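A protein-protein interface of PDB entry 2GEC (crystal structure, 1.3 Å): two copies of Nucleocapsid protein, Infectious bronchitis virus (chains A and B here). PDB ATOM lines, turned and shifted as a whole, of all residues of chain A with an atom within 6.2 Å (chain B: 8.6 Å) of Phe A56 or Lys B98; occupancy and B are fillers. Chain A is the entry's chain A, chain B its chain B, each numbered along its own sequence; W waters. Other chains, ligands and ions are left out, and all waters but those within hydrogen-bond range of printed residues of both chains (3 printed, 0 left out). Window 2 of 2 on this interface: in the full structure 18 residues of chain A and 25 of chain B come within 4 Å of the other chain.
N of Phe A56 lies within hydrogen-bond range of O of Glu B31.
NH1 of Arg A63 sits at hydrogen-bond distance from O of Ala B96.
NH2 of Arg A63 sits at hydrogen-bond distance from O of Ala B97, 3.4 Å away.
O of Arg A55 lies within hydrogen-bond range of N of Val A66 (3.0 Å).
The side-chain hydroxyl (OG1) of Thr B43 is in hydrogen-bond range of the backbone carbonyl oxygen (O) of Lys B98 (3.5 Å).
The backbone carbonyl oxygen of Gln B46 lies within hydrogen-bond range of the backbone NH of Ala B97 (3.0 Å).
Glu B31 touches Ala A54 (O to O, 3.98 Å).
Ala A54 touches Gly B32.
CD of Lys B98 touches CB of Ala A54, at 3.7 Å.
Arg A55 touches Glu B31 (CA to O, 3.2 Å).
Lys B98 touches Phe A56.
Arg A63 touches Lys B98.
Of chain B, only Glu B31 (2.9 Å) and Lys B98 (3.95 Å) come within 4 Å of Phe A56.
Of chain A, only Ala A54, Phe A56 and Arg A63 come within 4 Å of Lys B98.
Printed residues of chain B within 4 Å of Ala A54: Glu B31, Gly B32 and Lys B98.
Of the printed residues of chain B, Arg A55 touches Glu B31.
Of the printed residues of chain A, Gly B32 touches Ala A54.
Of the printed residues of chain A, Glu B31 touches Ala A54, Arg A55 and Phe A56.
Of the printed residues of chain B, Arg A63 touches Ala B96, Ala B97 and Lys B98.
Lys B29 touches none of the printed residues of chain A.
Ala B100 touches none of the printed residues of chain A.
The nearest residue of chain B that does not touch Phe A56 is Gly B32 (4.9 Å).
Hydrophobic or aromatic side chains of chain A within 4 Å of the printed part of chain B: Ala A54 and Phe A56.
Printed residues of chain B that touch a printed residue of chain A: Glu B31, Gly B32, Ala B96, Ala B97 and Lys B98.
Among the printed residues, 9 pairs touch across the chains.
Among the printed residues, no Asp or Glu carboxylate lies within 4 Å of a Lys or Arg side-chain nitrogen of the other chain.
No position is printed for both chains.
Of the 9 pairs that touch across the chains among the printed residues, none has its exchanged pair printed and touching as well.
Water W1 bridges O of Ala A54 (2.6 Å) and O of Asp B125 (2.9 Å).
Water W2 lies within hydrogen-bond range of the backbone carbonyl oxygen (O) of Ser B33 (2.7 Å), the backbone NH (N) of Ala B96 (3.1 Å), the guanidinium group (NH1) of Arg A63 (3.2 Å) and the backbone carbonyl oxygen (O) of Gly B32 (3.4 Å).
Water W3 bridges the backbone NH (N) of Gly B99 (3.3 Å) and the guanidinium group (NH2) of Arg A63 (3.4 Å).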
ATOM      1  N   ALA A  54     -27.529 -25.865   3.382  1.00  0.00           N
ATOM      2  CA  ALA A  54     -26.273 -25.234   3.722  1.00  0.00           C
ATOM      3  C   ALA A  54     -26.041 -23.941   2.930  1.00  0.00           C
ATOM      4  O   ALA A  54     -26.414 -23.844   1.722  1.00  0.00           O
ATOM      5  CB  ALA A  54     -25.113 -26.158   3.539  1.00  0.00           C
ATOM      6  N   ARG A  55     -25.486 -22.940   3.574  1.00  0.00           N
ATOM      7  CA  ARG A  55     -25.158 -21.687   2.920  1.00  0.00           C
ATOM      8  C   ARG A  55     -23.677 -21.320   3.192  1.00  0.00           C
ATOM      9  O   ARG A  55     -23.102 -21.600   4.256  1.00  0.00           O
ATOM     10  CB  ARG A  55     -26.054 -20.599   3.462  1.00  0.00           C
ATOM     11  CG  ARG A  55     -27.518 -20.848   3.098  1.00  0.00           C
ATOM     12  CD  ARG A  55     -28.411 -19.651   3.392  1.00  0.00           C
ATOM     13  NE  ARG A  55     -28.289 -19.232   4.776  1.00  0.00           N
ATOM     14  CZ  ARG A  55     -28.378 -17.981   5.220  1.00  0.00           C
ATOM     15  NH1 ARG A  55     -28.677 -16.987   4.357  1.00  0.00           N
ATOM     16  NH2 ARG A  55     -28.169 -17.748   6.527  1.00  0.00           N
ATOM     17  N   PHE A  56     -23.113 -20.537   2.287  1.00  0.00           N
ATOM     18  CA  PHE A  56     -21.753 -20.072   2.389  1.00  0.00           C
ATOM     19  C   PHE A  56     -21.639 -18.676   1.887  1.00  0.00           C
ATOM     20  O   PHE A  56     -22.567 -18.158   1.217  1.00  0.00           O
ATOM     21  CB  PHE A  56     -20.885 -20.922   1.514  1.00  0.00           C
ATOM     22  CG  PHE A  56     -20.898 -22.345   1.886  1.00  0.00           C
ATOM     23  CD1 PHE A  56     -19.961 -22.832   2.775  1.00  0.00           C
ATOM     24  CD2 PHE A  56     -21.824 -23.198   1.332  1.00  0.00           C
ATOM     25  CE1 PHE A  56     -19.959 -24.120   3.169  1.00  0.00           C
ATOM     26  CE2 PHE A  56     -21.846 -24.557   1.725  1.00  0.00           C
ATOM     27  CZ  PHE A  56     -20.881 -25.014   2.653  1.00  0.00           C
ATOM     28  N   LYS A  57     -20.471 -18.079   2.246  1.00  0.00           N
ATOM     29  CA  LYS A  57     -20.118 -16.731   1.773  1.00  0.00           C
ATOM     30  C   LYS A  57     -18.700 -16.752   1.204  1.00  0.00           C
ATOM     31  O   LYS A  57     -17.907 -17.686   1.537  1.00  0.00           O
ATOM     32  CB  LYS A  57     -20.211 -15.693   2.935  1.00  0.00           C
ATOM     33  CG  LYS A  57     -19.304 -16.012   4.116  1.00  0.00           C
ATOM     34  CD  LYS A  57     -19.238 -14.919   5.182  1.00  0.00           C
ATOM     35  CE  LYS A  57     -18.340 -15.293   6.331  1.00  0.00           C
ATOM     36  NZ  LYS A  57     -18.745 -14.437   7.508  1.00  0.00           N
ATOM     37  N   PRO A  58     -18.372 -15.751   0.339  1.00  0.00           N
ATOM     38  CA  PRO A  58     -17.037 -15.367  -0.036  1.00  0.00           C
ATOM     39  C   PRO A  58     -16.396 -14.660   1.172  1.00  0.00           C
ATOM     40  O   PRO A  58     -17.037 -13.778   1.800  1.00  0.00           O
ATOM     41  CB  PRO A  58     -17.245 -14.419  -1.220  1.00  0.00           C
ATOM     42  CG  PRO A  58     -18.628 -13.833  -1.042  1.00  0.00           C
ATOM     43  CD  PRO A  58     -19.402 -14.829  -0.191  1.00  0.00           C
ATOM     44  N   ARG A  63     -14.372 -20.449   0.372  1.00  0.00           N
ATOM     45  CA  ARG A  63     -15.697 -20.047   0.912  1.00  0.00           C
ATOM     46  C   ARG A  63     -15.814 -20.396   2.363  1.00  0.00           C
ATOM     47  O   ARG A  63     -15.200 -21.378   2.786  1.00  0.00           O
ATOM     48  CB  ARG A  63     -16.809 -20.759   0.151  1.00  0.00           C
ATOM     49  CG  ARG A  63     -16.810 -22.308   0.281  1.00  0.00           C
ATOM     50  CD  ARG A  63     -18.013 -22.845  -0.623  1.00  0.00           C
ATOM     51  NE  ARG A  63     -18.238 -24.279  -0.446  1.00  0.00           N
ATOM     52  CZ  ARG A  63     -18.978 -25.009  -1.277  1.00  0.00           C
ATOM     53  NH1 ARG A  63     -19.597 -24.427  -2.289  1.00  0.00           N
ATOM     54  NH2 ARG A  63     -19.096 -26.310  -1.124  1.00  0.00           N
ATOM     55  N   LYS A  64     -16.629 -19.610   3.099  1.00  0.00           N
ATOM     56  CA  LYS A  64     -16.842 -19.824   4.569  1.00  0.00           C
ATOM     57  C   LYS A  64     -18.295 -20.136   4.854  1.00  0.00           C
ATOM     58  O   LYS A  64     -19.146 -19.560   4.190  1.00  0.00           O
ATOM     59  CB  LYS A  64     -16.543 -18.516   5.324  1.00  0.00           C
ATOM     60  CG  LYS A  64     -16.522 -18.605   6.832  1.00  0.00           C
ATOM     61  CD  LYS A  64     -15.876 -19.904   7.197  1.00  0.00           C
ATOM     62  CE  LYS A  64     -14.891 -19.645   8.277  1.00  0.00           C
ATOM     63  NZ  LYS A  64     -13.593 -20.469   8.033  1.00  0.00           N
ATOM     64  N   PRO A  65     -18.561 -21.058   5.792  1.00  0.00           N
ATOM     65  CA  PRO A  65     -19.969 -21.319   6.105  1.00  0.00           C
ATOM     66  C   PRO A  65     -20.725 -20.184   6.760  1.00  0.00           C
ATOM     67  O   PRO A  65     -20.125 -19.422   7.501  1.00  0.00           O
ATOM     68  CB  PRO A  65     -19.892 -22.492   7.075  1.00  0.00           C
ATOM     69  CG  PRO A  65     -18.494 -22.499   7.590  1.00  0.00           C
ATOM     70  CD  PRO A  65     -17.617 -21.953   6.503  1.00  0.00           C
ATOM     71  N   VAL A  66     -22.016 -20.065   6.532  1.00  0.00           N
ATOM     72  CA  VAL A  66     -22.839 -19.187   7.311  1.00  0.00           C
ATOM     73  C   VAL A  66     -24.046 -20.026   7.783  1.00  0.00           C
ATOM     74  O   VAL A  66     -24.187 -21.167   7.415  1.00  0.00           O
ATOM     75  CB  VAL A  66     -23.254 -17.903   6.538  1.00  0.00           C
ATOM     76  CG1 VAL A  66     -22.024 -17.196   5.986  1.00  0.00           C
ATOM     77  CG2 VAL A  66     -24.206 -18.302   5.404  1.00  0.00           C
ATOM     78  N   LYS B  29     -24.253 -15.473  -8.416  1.00  0.00           N
ATOM     79  CA  LYS B  29     -23.764 -15.816  -7.108  1.00  0.00           C
ATOM     80  C   LYS B  29     -24.609 -16.938  -6.538  1.00  0.00           C
ATOM     81  O   LYS B  29     -25.825 -16.963  -6.744  1.00  0.00           O
ATOM     82  CB  LYS B  29     -24.005 -14.602  -6.139  1.00  0.00           C
ATOM     83  CG  LYS B  29     -23.295 -13.322  -6.530  1.00  0.00           C
ATOM     84  CD  LYS B  29     -23.682 -12.211  -5.487  1.00  0.00           C
ATOM     85  CE  LYS B  29     -23.609 -12.757  -4.098  1.00  0.00           C
ATOM     86  NZ  LYS B  29     -23.324 -11.561  -3.173  1.00  0.00           N
ATOM     87  N   PHE B  30     -23.927 -17.854  -5.838  1.00  0.00           N
ATOM     88  CA  PHE B  30     -24.625 -19.071  -5.374  1.00  0.00           C
ATOM     89  C   PHE B  30     -24.335 -19.220  -3.875  1.00  0.00           C
ATOM     90  O   PHE B  30     -23.172 -19.605  -3.524  1.00  0.00           O
ATOM     91  CB  PHE B  30     -24.118 -20.306  -6.088  1.00  0.00           C
ATOM     92  CG  PHE B  30     -24.297 -20.231  -7.583  1.00  0.00           C
ATOM     93  CD1 PHE B  30     -23.320 -19.711  -8.409  1.00  0.00           C
ATOM     94  CD2 PHE B  30     -25.543 -20.699  -8.199  1.00  0.00           C
ATOM     95  CE1 PHE B  30     -23.501 -19.637  -9.811  1.00  0.00           C
ATOM     96  CE2 PHE B  30     -25.715 -20.681  -9.613  1.00  0.00           C
ATOM     97  CZ  PHE B  30     -24.678 -20.113 -10.421  1.00  0.00           C
ATOM     98  N   GLU B  31     -25.272 -18.843  -2.999  1.00  0.00           N
ATOM     99  CA  GLU B  31     -25.109 -18.995  -1.545  1.00  0.00           C
ATOM    100  C   GLU B  31     -25.207 -20.429  -1.136  1.00  0.00           C
ATOM    101  O   GLU B  31     -24.636 -20.813  -0.137  1.00  0.00           O
ATOM    102  CB  GLU B  31     -26.245 -18.193  -0.864  1.00  0.00           C
ATOM    103  N   GLY B  32     -25.979 -21.241  -1.867  1.00  0.00           N
ATOM    104  CA  GLY B  32     -26.018 -22.713  -1.602  1.00  0.00           C
ATOM    105  C   GLY B  32     -25.148 -23.347  -2.672  1.00  0.00           C
ATOM    106  O   GLY B  32     -24.079 -22.863  -2.978  1.00  0.00           O
ATOM    107  N   SER B  33     -25.516 -24.511  -3.133  1.00  0.00           N
ATOM    108  CA  SER B  33     -24.602 -25.313  -3.993  1.00  0.00           C
ATOM    109  C   SER B  33     -24.465 -24.716  -5.352  1.00  0.00           C
ATOM    110  O   SER B  33     -23.357 -24.641  -5.900  1.00  0.00           O
ATOM    111  CB  SER B  33     -25.066 -26.768  -4.108  1.00  0.00           C
ATOM    112  OG  SER B  33     -26.119 -26.924  -4.951  1.00  0.00           O
ATOM    113  N   GLY B  34     -25.555 -24.294  -6.005  1.00  0.00           N
ATOM    114  CA  GLY B  34     -25.495 -23.859  -7.452  1.00  0.00           C
ATOM    115  C   GLY B  34     -25.314 -25.042  -8.427  1.00  0.00           C
ATOM    116  O   GLY B  34     -25.153 -24.804  -9.601  1.00  0.00           O
ATOM    117  N   VAL B  35     -25.450 -26.277  -7.944  1.00  0.00           N
ATOM    118  CA  VAL B  35     -25.269 -27.430  -8.795  1.00  0.00           C
ATOM    119  C   VAL B  35     -26.676 -27.957  -9.119  1.00  0.00           C
ATOM    120  O   VAL B  35     -27.499 -28.215  -8.182  1.00  0.00           O
ATOM    121  CB  VAL B  35     -24.434 -28.531  -8.058  1.00  0.00           C
ATOM    122  CG1 VAL B  35     -24.371 -29.790  -8.944  1.00  0.00           C
ATOM    123  CG2 VAL B  35     -23.056 -27.999  -7.713  1.00  0.00           C
ATOM    124  N   LYS B  42     -23.525 -38.946  -6.772  1.00  0.00           N
ATOM    125  CA  LYS B  42     -23.516 -38.836  -5.322  1.00  0.00           C
ATOM    126  C   LYS B  42     -23.041 -37.444  -4.966  1.00  0.00           C
ATOM    127  O   LYS B  42     -22.403 -36.776  -5.746  1.00  0.00           O
ATOM    128  CB  LYS B  42     -22.551 -39.936  -4.753  1.00  0.00           C
ATOM    129  CG  LYS B  42     -23.223 -41.281  -4.886  1.00  0.00           C
ATOM    130  N   THR B  43     -23.242 -37.011  -3.715  1.00  0.00           N
ATOM    131  CA  THR B  43     -22.838 -35.720  -3.200  1.00  0.00           C
ATOM    132  C   THR B  43     -21.339 -35.436  -3.538  1.00  0.00           C
ATOM    133  O   THR B  43     -21.000 -34.306  -3.964  1.00  0.00           O
ATOM    134  CB  THR B  43     -23.187 -35.643  -1.686  1.00  0.00           C
ATOM    135  OG1 THR B  43     -22.642 -34.409  -1.243  1.00  0.00           O
ATOM    136  CG2 THR B  43     -22.501 -36.741  -0.956  1.00  0.00           C
ATOM    137  N   SER B  44     -20.456 -36.436  -3.456  1.00  0.00           N
ATOM    138  CA  SER B  44     -19.040 -36.154  -3.679  1.00  0.00           C
ATOM    139  C   SER B  44     -18.770 -35.681  -5.071  1.00  0.00           C
ATOM    140  O   SER B  44     -17.775 -34.948  -5.263  1.00  0.00           O
ATOM    141  CB  SER B  44     -18.210 -37.411  -3.428  1.00  0.00           C
ATOM    142  OG  SER B  44     -18.764 -38.563  -4.076  1.00  0.00           O
ATOM    143  N   GLN B  45     -19.670 -35.980  -6.021  1.00  0.00           N
ATOM    144  CA  GLN B  45     -19.488 -35.690  -7.444  1.00  0.00           C
ATOM    145  C   GLN B  45     -20.163 -34.396  -7.905  1.00  0.00           C
ATOM    146  O   GLN B  45     -20.114 -34.055  -9.044  1.00  0.00           O
ATOM    147  CB  GLN B  45     -20.128 -36.828  -8.233  1.00  0.00           C
ATOM    148  CG  GLN B  45     -19.435 -38.181  -8.091  1.00  0.00           C
ATOM    149  CD  GLN B  45     -20.217 -39.290  -8.762  1.00  0.00           C
ATOM    150  OE1 GLN B  45     -21.249 -39.671  -8.317  1.00  0.00           O
ATOM    151  NE2 GLN B  45     -19.675 -39.795  -9.802  1.00  0.00           N
ATOM    152  N   GLN B  46     -20.811 -33.713  -6.984  1.00  0.00           N
ATOM    153  CA  GLN B  46     -21.724 -32.618  -7.325  1.00  0.00           C
ATOM    154  C   GLN B  46     -20.917 -31.321  -7.321  1.00  0.00           C
ATOM    155  O   GLN B  46     -20.908 -30.600  -6.398  1.00  0.00           O
ATOM    156  CB  GLN B  46     -22.887 -32.586  -6.331  1.00  0.00           C
ATOM    157  CG  GLN B  46     -23.978 -33.708  -6.554  1.00  0.00           C
ATOM    158  CD  GLN B  46     -24.712 -33.630  -7.976  1.00  0.00           C
ATOM    159  N   HIS B  47     -20.227 -31.096  -8.419  1.00  0.00           N
ATOM    160  CA  HIS B  47     -19.421 -29.897  -8.594  1.00  0.00           C
ATOM    161  C   HIS B  47     -19.204 -29.609 -10.072  1.00  0.00           C
ATOM    162  O   HIS B  47     -19.204 -30.525 -10.875  1.00  0.00           O
ATOM    163  CB  HIS B  47     -18.072 -30.040  -7.860  1.00  0.00           C
ATOM    164  CG  HIS B  47     -17.203 -31.156  -8.358  1.00  0.00           C
ATOM    165  ND1 HIS B  47     -17.215 -32.418  -7.826  1.00  0.00           N
ATOM    166  CD2 HIS B  47     -16.296 -31.180  -9.349  1.00  0.00           C
ATOM    167  CE1 HIS B  47     -16.357 -33.172  -8.480  1.00  0.00           C
ATOM    168  NE2 HIS B  47     -15.768 -32.430  -9.377  1.00  0.00           N
ATOM    169  N   VAL B  95     -18.924 -23.978  -8.734  1.00  0.00           N
ATOM    170  CA  VAL B  95     -19.949 -24.381  -7.785  1.00  0.00           C
ATOM    171  C   VAL B  95     -19.669 -25.741  -7.271  1.00  0.00           C
ATOM    172  O   VAL B  95     -19.157 -26.665  -7.961  1.00  0.00           O
ATOM    173  CB  VAL B  95     -21.396 -24.269  -8.441  1.00  0.00           C
ATOM    174  CG1 VAL B  95     -21.780 -22.822  -8.666  1.00  0.00           C
ATOM    175  CG2 VAL B  95     -21.456 -25.024  -9.743  1.00  0.00           C
ATOM    176  N   ALA B  96     -20.075 -25.998  -6.066  1.00  0.00           N
ATOM    177  CA  ALA B  96     -19.949 -27.350  -5.444  1.00  0.00           C
ATOM    178  C   ALA B  96     -20.917 -27.502  -4.279  1.00  0.00           C
ATOM    179  O   ALA B  96     -21.132 -26.530  -3.513  1.00  0.00           O
ATOM    180  CB  ALA B  96     -18.539 -27.600  -4.973  1.00  0.00           C
ATOM    181  N   ALA B  97     -21.484 -28.712  -4.161  1.00  0.00           N
ATOM    182  CA  ALA B  97     -22.351 -28.994  -3.021  1.00  0.00           C
ATOM    183  C   ALA B  97     -21.486 -29.012  -1.776  1.00  0.00           C
ATOM    184  O   ALA B  97     -20.294 -29.385  -1.846  1.00  0.00           O
ATOM    185  CB  ALA B  97     -23.035 -30.332  -3.187  1.00  0.00           C
ATOM    186  N   LYS B  98     -22.106 -28.739  -0.610  1.00  0.00           N
ATOM    187  CA  LYS B  98     -21.413 -29.031   0.645  1.00  0.00           C
ATOM    188  C   LYS B  98     -21.038 -30.560   0.616  1.00  0.00           C
ATOM    189  O   LYS B  98     -21.897 -31.436   0.358  1.00  0.00           O
ATOM    190  CB  LYS B  98     -22.278 -28.627   1.880  1.00  0.00           C
ATOM    191  CG  LYS B  98     -21.715 -29.126   3.197  1.00  0.00           C
ATOM    192  CD  LYS B  98     -22.533 -28.599   4.409  1.00  0.00           C
ATOM    193  CE  LYS B  98     -21.853 -29.126   5.703  1.00  0.00           C
ATOM    194  NZ  LYS B  98     -21.767 -30.620   5.729  1.00  0.00           N
ATOM    195  N   GLY B  99     -19.790 -30.902   0.864  1.00  0.00           N
ATOM    196  CA  GLY B  99     -19.405 -32.297   0.850  1.00  0.00           C
ATOM    197  C   GLY B  99     -18.859 -32.797  -0.508  1.00  0.00           C
ATOM    198  O   GLY B  99     -18.467 -33.951  -0.653  1.00  0.00           O
ATOM    199  N   ALA B 100     -18.846 -31.950  -1.530  1.00  0.00           N
ATOM    200  CA  ALA B 100     -18.208 -32.343  -2.762  1.00  0.00           C
ATOM    201  C   ALA B 100     -16.688 -32.594  -2.601  1.00  0.00           C
ATOM    202  O   ALA B 100     -16.052 -31.885  -1.849  1.00  0.00           O
ATOM    203  CB  ALA B 100     -18.487 -31.335  -3.842  1.00  0.00           C
ATOM    204  N   ASP B 101     -16.181 -33.577  -3.365  1.00  0.00           N
ATOM    205  CA  ASP B 101     -14.742 -33.737  -3.550  1.00  0.00           C
ATOM    206  C   ASP B 101     -14.454 -33.202  -4.940  1.00  0.00           C
ATOM    207  O   ASP B 101     -14.736 -33.898  -5.907  1.00  0.00           O
ATOM    208  CB  ASP B 101     -14.365 -35.209  -3.510  1.00  0.00           C
ATOM    209  CG  ASP B 101     -12.899 -35.479  -3.858  1.00  0.00           C
ATOM    210  OD1 ASP B 101     -12.542 -36.677  -3.911  1.00  0.00           O
ATOM    211  OD2 ASP B 101     -12.139 -34.494  -4.138  1.00  0.00           O
ATOM    212  N   ASP B 125     -30.514 -27.513  -3.527  1.00  0.00           N
ATOM    213  CA  ASP B 125     -29.598 -26.998  -2.547  1.00  0.00           C
ATOM    214  C   ASP B 125     -29.213 -25.558  -2.816  1.00  0.00           C
ATOM    215  O   ASP B 125     -28.222 -25.071  -2.257  1.00  0.00           O
ATOM    216  CB  ASP B 125     -28.395 -27.930  -2.477  1.00  0.00           C
ATOM    217  CG  ASP B 125     -28.749 -29.293  -2.018  1.00  0.00           C
ATOM    218  OD1 ASP B 125     -28.129 -30.232  -2.539  1.00  0.00           O
ATOM    219  OD2 ASP B 125     -29.636 -29.450  -1.130  1.00  0.00           O
HETATM  220  O   HOH W   1     -26.479 -25.833  -0.013  1.00  0.00           O
HETATM  221  O   HOH W   2     -21.293 -23.420  -4.772  1.00  0.00           O
HETATM  222  O   HOH W   3     -17.787 -28.356   1.225  1.00  0.00           O
